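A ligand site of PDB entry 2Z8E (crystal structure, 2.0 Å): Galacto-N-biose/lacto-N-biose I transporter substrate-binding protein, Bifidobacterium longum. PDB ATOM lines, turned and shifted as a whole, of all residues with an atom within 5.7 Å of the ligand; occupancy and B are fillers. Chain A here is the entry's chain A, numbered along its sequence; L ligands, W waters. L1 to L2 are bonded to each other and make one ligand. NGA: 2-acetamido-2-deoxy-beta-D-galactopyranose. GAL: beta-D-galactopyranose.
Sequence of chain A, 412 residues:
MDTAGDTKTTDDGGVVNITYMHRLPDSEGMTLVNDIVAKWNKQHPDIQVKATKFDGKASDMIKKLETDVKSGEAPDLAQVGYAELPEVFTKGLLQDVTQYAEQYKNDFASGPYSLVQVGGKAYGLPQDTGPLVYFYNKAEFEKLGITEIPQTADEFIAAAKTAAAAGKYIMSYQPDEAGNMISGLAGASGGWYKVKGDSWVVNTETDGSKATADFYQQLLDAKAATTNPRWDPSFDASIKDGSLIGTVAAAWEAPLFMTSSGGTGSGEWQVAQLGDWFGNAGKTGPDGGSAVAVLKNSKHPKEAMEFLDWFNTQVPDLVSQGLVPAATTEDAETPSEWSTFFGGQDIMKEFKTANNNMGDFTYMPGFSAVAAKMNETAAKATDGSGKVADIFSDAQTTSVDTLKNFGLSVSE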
ATOM      1  N   ARG A  23     -20.703  -5.240   0.681  1.00  0.00           N
ATOM      2  CA  ARG A  23     -22.008  -4.581   0.812  1.00  0.00           C
ATOM      3  C   ARG A  23     -21.922  -3.516   1.887  1.00  0.00           C
ATOM      4  O   ARG A  23     -22.822  -3.306   2.720  1.00  0.00           O
ATOM      5  CB  ARG A  23     -23.165  -5.593   0.970  1.00  0.00           C
ATOM      6  CG  ARG A  23     -23.060  -6.673   2.086  1.00  0.00           C
ATOM      7  CD  ARG A  23     -24.260  -7.612   1.995  1.00  0.00           C
ATOM      8  NE  ARG A  23     -24.255  -8.777   2.895  1.00  0.00           N
ATOM      9  CZ  ARG A  23     -24.541  -8.744   4.194  1.00  0.00           C
ATOM     10  NH1 ARG A  23     -24.819  -7.607   4.814  1.00  0.00           N
ATOM     11  NH2 ARG A  23     -24.533  -9.860   4.889  1.00  0.00           N
ATOM     12  N   LEU A  24     -20.785  -2.825   1.883  1.00  0.00           N
ATOM     13  CA  LEU A  24     -20.584  -1.723   2.791  1.00  0.00           C
ATOM     14  C   LEU A  24     -21.301  -0.483   2.258  1.00  0.00           C
ATOM     15  O   LEU A  24     -21.418  -0.328   1.037  1.00  0.00           O
ATOM     16  CB  LEU A  24     -19.092  -1.479   2.996  1.00  0.00           C
ATOM     17  CG  LEU A  24     -18.324  -2.672   3.663  1.00  0.00           C
ATOM     18  CD1 LEU A  24     -16.904  -2.199   3.906  1.00  0.00           C
ATOM     19  CD2 LEU A  24     -18.955  -3.115   4.955  1.00  0.00           C
ATOM     20  N   PRO A  25     -21.809   0.378   3.183  1.00  0.00           N
ATOM     21  CA  PRO A  25     -22.708   1.452   2.727  1.00  0.00           C
ATOM     22  C   PRO A  25     -22.137   2.419   1.657  1.00  0.00           C
ATOM     23  O   PRO A  25     -22.855   2.751   0.723  1.00  0.00           O
ATOM     24  CB  PRO A  25     -23.002   2.258   4.001  1.00  0.00           C
ATOM     25  CG  PRO A  25     -21.970   1.755   5.035  1.00  0.00           C
ATOM     26  CD  PRO A  25     -21.668   0.349   4.647  1.00  0.00           C
ATOM     27  N   LYS A  57     -30.505  -5.701  -2.160  1.00  0.00           N
ATOM     28  CA  LYS A  57     -30.876  -5.819  -0.741  1.00  0.00           C
ATOM     29  C   LYS A  57     -29.854  -6.765  -0.066  1.00  0.00           C
ATOM     30  O   LYS A  57     -29.537  -7.843  -0.604  1.00  0.00           O
ATOM     31  CB  LYS A  57     -32.275  -6.433  -0.695  1.00  0.00           C
ATOM     32  CG  LYS A  57     -32.981  -6.488   0.640  1.00  0.00           C
ATOM     33  CD  LYS A  57     -34.136  -7.494   0.554  1.00  0.00           C
ATOM     34  CE  LYS A  57     -34.919  -7.589   1.866  1.00  0.00           C
ATOM     35  NZ  LYS A  57     -34.166  -8.079   3.066  1.00  0.00           N
ATOM     36  N   ALA A  58     -29.364  -6.381   1.119  1.00  0.00           N
ATOM     37  CA  ALA A  58     -28.287  -7.155   1.781  1.00  0.00           C
ATOM     38  C   ALA A  58     -28.457  -8.683   1.728  1.00  0.00           C
ATOM     39  O   ALA A  58     -27.544  -9.372   1.291  1.00  0.00           O
ATOM     40  CB  ALA A  58     -28.033  -6.648   3.225  1.00  0.00           C
ATOM     41  N   SER A  59     -29.617  -9.203   2.133  1.00  0.00           N
ATOM     42  CA  SER A  59     -29.872 -10.664   2.205  1.00  0.00           C
ATOM     43  C   SER A  59     -29.883 -11.370   0.846  1.00  0.00           C
ATOM     44  O   SER A  59     -29.919 -12.604   0.807  1.00  0.00           O
ATOM     45  CB  SER A  59     -31.195 -10.994   2.933  1.00  0.00           C
ATOM     46  OG  SER A  59     -32.330 -10.447   2.236  1.00  0.00           O
ATOM     47  N   GLN A  79     -18.047 -10.239   0.964  1.00  0.00           N
ATOM     48  CA  GLN A  79     -18.585 -10.084   2.310  1.00  0.00           C
ATOM     49  C   GLN A  79     -19.623 -11.178   2.602  1.00  0.00           C
ATOM     50  O   GLN A  79     -20.536 -11.447   1.804  1.00  0.00           O
ATOM     51  CB  GLN A  79     -19.142  -8.668   2.485  1.00  0.00           C
ATOM     52  CG  GLN A  79     -19.715  -8.426   3.873  1.00  0.00           C
ATOM     53  CD  GLN A  79     -20.246  -7.041   4.017  1.00  0.00           C
ATOM     54  OE1 GLN A  79     -19.974  -6.182   3.192  1.00  0.00           O
ATOM     55  NE2 GLN A  79     -21.033  -6.805   5.087  1.00  0.00           N
ATOM     56  N   GLU A  84     -24.382 -16.018   7.893  1.00  0.00           N
ATOM     57  CA  GLU A  84     -24.479 -16.602   6.529  1.00  0.00           C
ATOM     58  C   GLU A  84     -23.354 -17.588   6.209  1.00  0.00           C
ATOM     59  O   GLU A  84     -23.436 -18.341   5.235  1.00  0.00           O
ATOM     60  CB  GLU A  84     -24.390 -15.502   5.469  1.00  0.00           C
ATOM     61  CG  GLU A  84     -25.599 -14.528   5.475  1.00  0.00           C
ATOM     62  CD  GLU A  84     -25.373 -13.331   4.567  1.00  0.00           C
ATOM     63  OE1 GLU A  84     -24.206 -12.883   4.458  1.00  0.00           O
ATOM     64  OE2 GLU A  84     -26.361 -12.815   3.977  1.00  0.00           O
ATOM     65  N   GLN A 127     -14.431  -9.123   9.912  1.00  0.00           N
ATOM     66  CA  GLN A 127     -14.309  -7.723   9.569  1.00  0.00           C
ATOM     67  C   GLN A 127     -14.891  -6.825  10.636  1.00  0.00           C
ATOM     68  O   GLN A 127     -14.275  -5.785  10.977  1.00  0.00           O
ATOM     69  CB  GLN A 127     -14.911  -7.429   8.173  1.00  0.00           C
ATOM     70  CG  GLN A 127     -14.778  -6.019   7.741  1.00  0.00           C
ATOM     71  CD  GLN A 127     -15.226  -5.789   6.290  1.00  0.00           C
ATOM     72  OE1 GLN A 127     -16.434  -5.615   6.010  1.00  0.00           O
ATOM     73  NE2 GLN A 127     -14.260  -5.813   5.349  1.00  0.00           N
ATOM     74  N   ASP A 128     -16.058  -7.192  11.184  1.00  0.00           N
ATOM     75  CA  ASP A 128     -16.714  -6.305  12.163  1.00  0.00           C
ATOM     76  C   ASP A 128     -17.645  -7.078  13.090  1.00  0.00           C
ATOM     77  O   ASP A 128     -17.839  -8.244  12.920  1.00  0.00           O
ATOM     78  CB  ASP A 128     -17.527  -5.196  11.444  1.00  0.00           C
ATOM     79  CG  ASP A 128     -18.700  -5.753  10.613  1.00  0.00           C
ATOM     80  OD1 ASP A 128     -18.495  -6.694   9.821  1.00  0.00           O
ATOM     81  OD2 ASP A 128     -19.840  -5.276  10.780  1.00  0.00           O
ATOM     82  N   GLU A 177     -36.704  -6.451   9.719  1.00  0.00           N
ATOM     83  CA  GLU A 177     -35.440  -6.796  10.374  1.00  0.00           C
ATOM     84  C   GLU A 177     -35.623  -7.802  11.507  1.00  0.00           C
ATOM     85  O   GLU A 177     -34.669  -8.052  12.251  1.00  0.00           O
ATOM     86  CB  GLU A 177     -34.729  -5.536  10.911  1.00  0.00           C
ATOM     87  CG  GLU A 177     -33.989  -4.711   9.796  1.00  0.00           C
ATOM     88  CD  GLU A 177     -32.810  -5.481   9.198  1.00  0.00           C
ATOM     89  OE1 GLU A 177     -32.098  -6.160   9.975  1.00  0.00           O
ATOM     90  OE2 GLU A 177     -32.589  -5.404   7.957  1.00  0.00           O
ATOM     91  N   ASN A 180     -32.944 -10.597  11.856  1.00  0.00           N
ATOM     92  CA  ASN A 180     -31.593 -10.217  12.255  1.00  0.00           C
ATOM     93  C   ASN A 180     -31.612  -9.590  13.660  1.00  0.00           C
ATOM     94  O   ASN A 180     -30.756  -9.896  14.513  1.00  0.00           O
ATOM     95  CB  ASN A 180     -31.018  -9.211  11.256  1.00  0.00           C
ATOM     96  CG  ASN A 180     -30.926  -9.778   9.816  1.00  0.00           C
ATOM     97  OD1 ASN A 180     -30.661 -10.952   9.609  1.00  0.00           O
ATOM     98  ND2 ASN A 180     -31.149  -8.902   8.823  1.00  0.00           N
ATOM     99  N   TRP A 231     -36.018  -0.035   6.552  1.00  0.00           N
ATOM    100  CA  TRP A 231     -35.415   0.404   5.282  1.00  0.00           C
ATOM    101  C   TRP A 231     -36.384   1.199   4.382  1.00  0.00           C
ATOM    102  O   TRP A 231     -36.010   1.641   3.283  1.00  0.00           O
ATOM    103  CB  TRP A 231     -34.765  -0.794   4.545  1.00  0.00           C
ATOM    104  CG  TRP A 231     -33.874  -1.531   5.483  1.00  0.00           C
ATOM    105  CD1 TRP A 231     -34.005  -2.837   5.885  1.00  0.00           C
ATOM    106  CD2 TRP A 231     -32.770  -0.972   6.234  1.00  0.00           C
ATOM    107  NE1 TRP A 231     -33.032  -3.121   6.855  1.00  0.00           N
ATOM    108  CE2 TRP A 231     -32.285  -1.997   7.082  1.00  0.00           C
ATOM    109  CE3 TRP A 231     -32.181   0.287   6.289  1.00  0.00           C
ATOM    110  CZ2 TRP A 231     -31.194  -1.798   7.951  1.00  0.00           C
ATOM    111  CZ3 TRP A 231     -31.085   0.484   7.144  1.00  0.00           C
ATOM    112  CH2 TRP A 231     -30.625  -0.555   7.985  1.00  0.00           C
ATOM    113  N   TRP A 252     -23.534  -0.793  14.050  1.00  0.00           N
ATOM    114  CA  TRP A 252     -23.115  -0.368  12.680  1.00  0.00           C
ATOM    115  C   TRP A 252     -24.159   0.615  12.053  1.00  0.00           C
ATOM    116  O   TRP A 252     -23.900   1.248  11.004  1.00  0.00           O
ATOM    117  CB  TRP A 252     -22.770  -1.553  11.734  1.00  0.00           C
ATOM    118  CG  TRP A 252     -23.775  -2.681  11.745  1.00  0.00           C
ATOM    119  CD1 TRP A 252     -23.656  -3.898  12.398  1.00  0.00           C
ATOM    120  CD2 TRP A 252     -25.062  -2.689  11.117  1.00  0.00           C
ATOM    121  NE1 TRP A 252     -24.794  -4.663  12.191  1.00  0.00           N
ATOM    122  CE2 TRP A 252     -25.668  -3.929  11.428  1.00  0.00           C
ATOM    123  CE3 TRP A 252     -25.784  -1.756  10.323  1.00  0.00           C
ATOM    124  CZ2 TRP A 252     -26.945  -4.262  10.975  1.00  0.00           C
ATOM    125  CZ3 TRP A 252     -27.053  -2.084   9.872  1.00  0.00           C
ATOM    126  CH2 TRP A 252     -27.623  -3.318  10.210  1.00  0.00           C
ATOM    127  N   LEU A 256     -25.667   5.537   9.247  1.00  0.00           N
ATOM    128  CA  LEU A 256     -26.967   5.347   8.588  1.00  0.00           C
ATOM    129  C   LEU A 256     -28.087   6.151   9.242  1.00  0.00           C
ATOM    130  O   LEU A 256     -28.792   6.920   8.592  1.00  0.00           O
ATOM    131  CB  LEU A 256     -27.332   3.846   8.555  1.00  0.00           C
ATOM    132  CG  LEU A 256     -26.219   2.912   8.033  1.00  0.00           C
ATOM    133  CD1 LEU A 256     -26.628   1.460   7.984  1.00  0.00           C
ATOM    134  CD2 LEU A 256     -25.662   3.356   6.637  1.00  0.00           C
ATOM    135  N   ASP A 287     -26.554  -8.710  15.866  1.00  0.00           N
ATOM    136  CA  ASP A 287     -27.383  -8.364  14.742  1.00  0.00           C
ATOM    137  C   ASP A 287     -26.395  -8.019  13.594  1.00  0.00           C
ATOM    138  O   ASP A 287     -25.781  -6.942  13.571  1.00  0.00           O
ATOM    139  CB  ASP A 287     -28.269  -7.193  15.149  1.00  0.00           C
ATOM    140  CG  ASP A 287     -29.121  -6.667  14.020  1.00  0.00           C
ATOM    141  OD1 ASP A 287     -28.963  -7.148  12.868  1.00  0.00           O
ATOM    142  OD2 ASP A 287     -29.935  -5.742  14.307  1.00  0.00           O
ATOM    143  N   GLY A 288     -26.197  -8.939  12.675  1.00  0.00           N
ATOM    144  CA  GLY A 288     -25.258  -8.679  11.604  1.00  0.00           C
ATOM    145  C   GLY A 288     -23.830  -8.838  12.173  1.00  0.00           C
ATOM    146  O   GLY A 288     -23.645  -9.522  13.192  1.00  0.00           O
ATOM    147  N   GLY A 289     -22.853  -8.183  11.525  1.00  0.00           N
ATOM    148  CA  GLY A 289     -21.423  -8.480  11.748  1.00  0.00           C
ATOM    149  C   GLY A 289     -21.013  -9.469  10.675  1.00  0.00           C
ATOM    150  O   GLY A 289     -21.684 -10.487  10.477  1.00  0.00           O
ATOM    151  N   SER A 290     -19.920  -9.181   9.972  1.00  0.00           N
ATOM    152  CA  SER A 290     -19.577  -9.964   8.805  1.00  0.00           C
ATOM    153  C   SER A 290     -18.099 -10.332   8.759  1.00  0.00           C
ATOM    154  O   SER A 290     -17.254  -9.703   9.394  1.00  0.00           O
ATOM    155  CB  SER A 290     -19.947  -9.236   7.510  1.00  0.00           C
ATOM    156  OG  SER A 290     -21.209  -8.586   7.551  1.00  0.00           O
ATOM    157  N   GLN A 321     -17.334   3.743   7.810  1.00  0.00           N
ATOM    158  CA  GLN A 321     -18.437   3.001   7.216  1.00  0.00           C
ATOM    159  C   GLN A 321     -19.464   2.502   8.257  1.00  0.00           C
ATOM    160  O   GLN A 321     -20.417   1.759   7.942  1.00  0.00           O
ATOM    161  CB  GLN A 321     -17.851   1.836   6.442  1.00  0.00           C
ATOM    162  CG  GLN A 321     -16.946   2.234   5.247  1.00  0.00           C
ATOM    163  CD  GLN A 321     -17.721   2.503   3.957  1.00  0.00           C
ATOM    164  OE1 GLN A 321     -18.891   2.123   3.848  1.00  0.00           O
ATOM    165  NE2 GLN A 321     -17.061   3.099   2.959  1.00  0.00           N
ATOM    166  N   LEU A 323     -18.515   0.575  10.844  1.00  0.00           N
ATOM    167  CA  LEU A 323     -18.126  -0.724  11.405  1.00  0.00           C
ATOM    168  C   LEU A 323     -17.487  -0.607  12.786  1.00  0.00           C
ATOM    169  O   LEU A 323     -16.768   0.382  13.106  1.00  0.00           O
ATOM    170  CB  LEU A 323     -17.188  -1.503  10.464  1.00  0.00           C
ATOM    171  CG  LEU A 323     -17.647  -1.602   8.997  1.00  0.00           C
ATOM    172  CD1 LEU A 323     -16.700  -2.497   8.185  1.00  0.00           C
ATOM    173  CD2 LEU A 323     -19.052  -2.091   8.885  1.00  0.00           C
HETATM  174  C1  NGA L   1     -29.465  -5.304   7.003  1.00  0.00           C
HETATM  175  C2  NGA L   1     -28.089  -6.046   6.973  1.00  0.00           C
HETATM  176  C3  NGA L   1     -26.988  -5.016   7.157  1.00  0.00           C
HETATM  177  C4  NGA L   1     -27.138  -3.765   6.243  1.00  0.00           C
HETATM  178  C5  NGA L   1     -28.569  -3.205   6.302  1.00  0.00           C
HETATM  179  C6  NGA L   1     -28.766  -2.081   5.298  1.00  0.00           C
HETATM  180  C7  NGA L   1     -27.507  -8.270   7.790  1.00  0.00           C
HETATM  181  C8  NGA L   1     -27.532  -9.203   8.965  1.00  0.00           C
HETATM  182  N2  NGA L   1     -28.040  -7.072   8.029  1.00  0.00           N
HETATM  183  O1  NGA L   1     -30.424  -6.235   6.606  1.00  0.00           O
HETATM  184  O3  NGA L   1     -25.689  -5.644   7.035  1.00  0.00           O
HETATM  185  O4  NGA L   1     -26.725  -4.103   4.892  1.00  0.00           O
HETATM  186  O5  NGA L   1     -29.501  -4.254   6.055  1.00  0.00           O
HETATM  187  O6  NGA L   1     -27.989  -0.912   5.659  1.00  0.00           O
HETATM  188  O7  NGA L   1     -27.048  -8.593   6.683  1.00  0.00           O
HETATM  189  C1  GAL L   2     -24.719  -5.028   7.895  1.00  0.00           C
HETATM  190  C2  GAL L   2     -23.668  -6.070   8.297  1.00  0.00           C
HETATM  191  C3  GAL L   2     -22.521  -5.380   9.023  1.00  0.00           C
HETATM  192  C4  GAL L   2     -21.974  -4.188   8.223  1.00  0.00           C
HETATM  193  C5  GAL L   2     -23.121  -3.205   7.893  1.00  0.00           C
HETATM  194  C6  GAL L   2     -22.691  -2.173   6.866  1.00  0.00           C
HETATM  195  O2  GAL L   2     -24.238  -7.120   9.044  1.00  0.00           O
HETATM  196  O3  GAL L   2     -21.562  -6.383   9.239  1.00  0.00           O
HETATM  197  O4  GAL L   2     -21.443  -4.717   6.999  1.00  0.00           O
HETATM  198  O5  GAL L   2     -24.093  -3.985   7.201  1.00  0.00           O
HETATM  199  O6  GAL L   2     -23.449  -0.983   6.975  1.00  0.00           O
HETATM  200  O   HOH W   1     -31.583  -7.252   3.601  1.00  0.00           O
HETATM  201  O   HOH W   2     -24.072  -4.691   4.662  1.00  0.00           O
HETATM  202  O   HOH W   3     -24.100  -9.401   7.890  1.00  0.00           O
HETATM  203  O   HOH W   4     -29.381  -6.297  10.260  1.00  0.00           O
HETATM  204  O   HOH W   5     -22.860   0.885   8.635  1.00  0.00           O
HETATM  205  O   HOH W   6     -28.991   1.350   4.508  1.00  0.00           O
HETATM  206  O   HOH W   7     -27.055  -3.028   2.186  1.00  0.00           O
HETATM  207  O   HOH W   8     -30.372  -9.296   5.839  1.00  0.00           O
HETATM  208  O   HOH W   9     -18.858  -5.750   7.412  1.00  0.00           O
HETATM  209  O   HOH W  10     -27.752 -10.975   5.742  1.00  0.00           O
HETATM  210  O   HOH W  11     -25.411  -0.518   4.958  1.00  0.00           O
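An oxygen (O3) of GAL L2 lies within hydrogen-bond range of the side-chain carboxylate of Asp 128 (2.6 Å).
OE2 of Glu 177 sits at hydrogen-bond distance from O1 of NGA L1 (2.7 Å).
N of Ser 290 lies within hydrogen-bond range of O3 of GAL L2, at 3.3 Å.
The side-chain hydroxyl of Ser 290 lies within hydrogen-bond range of an oxygen (O3) of GAL L2 (2.8 Å).
The side-chain amide nitrogen (NE2) of Gln 79 is in hydrogen-bond range of an oxygen (O4) of GAL L2.
N of Gly 289 lies within hydrogen-bond range of O2 of GAL L2, at 3.0 Å.
O7 of NGA L1 sits at hydrogen-bond distance from NH1 of Arg 23 (3.1 Å).
The backbone NH (N) of Ser 290 is in hydrogen-bond range of the side-chain carboxylate (OD1) of Asp 128 (2.9 Å).
OE2 of Glu 177 sits at hydrogen-bond distance from NE1 of Trp 231, at 2.6 Å.
The side-chain carboxylate (OE1) of Glu 177 sits at hydrogen-bond distance from the side-chain amide nitrogen (ND2) of Asn 180.
The side-chain amide nitrogen of Gln 79 is in hydrogen-bond range of the side-chain hydroxyl of Ser 290.
The backbone NH (N) of Gln 127 is in hydrogen-bond range of the backbone carbonyl oxygen (O) of Ser 290.
OE1 of Gln 79 sits at hydrogen-bond distance from N of Arg 23 (2.8 Å).
The guanidinium group of Arg 23 is in salt-bridge range of the side-chain carboxylate of Glu 84, 3.1 Å away.
NE1 of Trp 252 sits at hydrogen-bond distance from O of Asp 287, at 2.8 Å.
CD2 of Leu 24 touches O4 of GAL L2, 3.6 Å away.
CD of Pro 25 touches O6 of GAL L2, at 3.2 Å.
Ala 58 touches the ligand.
ND2 of Asn 180 touches O1 of NGA L1, 3.5 Å away.
Trp 231 touches the ligand.
CH2 of Trp 252 touches C3 of NGA L1, 3.6 Å away.
Leu 256 touches the ligand.
CA of Gly 288 touches O2 of GAL L2 (3.2 Å).
CD2 of Leu 323 touches C4 of GAL L2, 3.7 Å away.
Water W3 lies within hydrogen-bond range of an oxygen (O2) of GAL L2 (2.6 Å), the side-chain hydroxyl (OG) of Ser 290 (3.0 Å) and the guanidinium group (NH2) of Arg 23 (3.1 Å).
Water W5 lies within hydrogen-bond range of an oxygen (O6) of GAL L2, the backbone carbonyl oxygen (O) of Trp 252 and the backbone carbonyl oxygen (O) of Gln 321.
Water W2 lies within hydrogen-bond range of O5 of GAL L2 (2.6 Å) and O of Arg 23 (2.7 Å).
Water W10 lies within hydrogen-bond range of an oxygen (O7) of NGA L1 (2.7 Å) and the side-chain carboxylate of Glu 84 (2.9 Å).
Water W4 lies within hydrogen-bond range of a nitrogen (N2) of NGA L1 (2.7 Å), the side-chain carboxylate of Glu 177 (2.7 Å), the side-chain carboxylate of Asp 287 (2.8 Å) and the side-chain amide nitrogen of Asn 180 (3.5 Å).
Water W8 lies within hydrogen-bond range of ND2 of Asn 180 (3.1 Å) and O1 of NGA L1 (3.2 Å).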
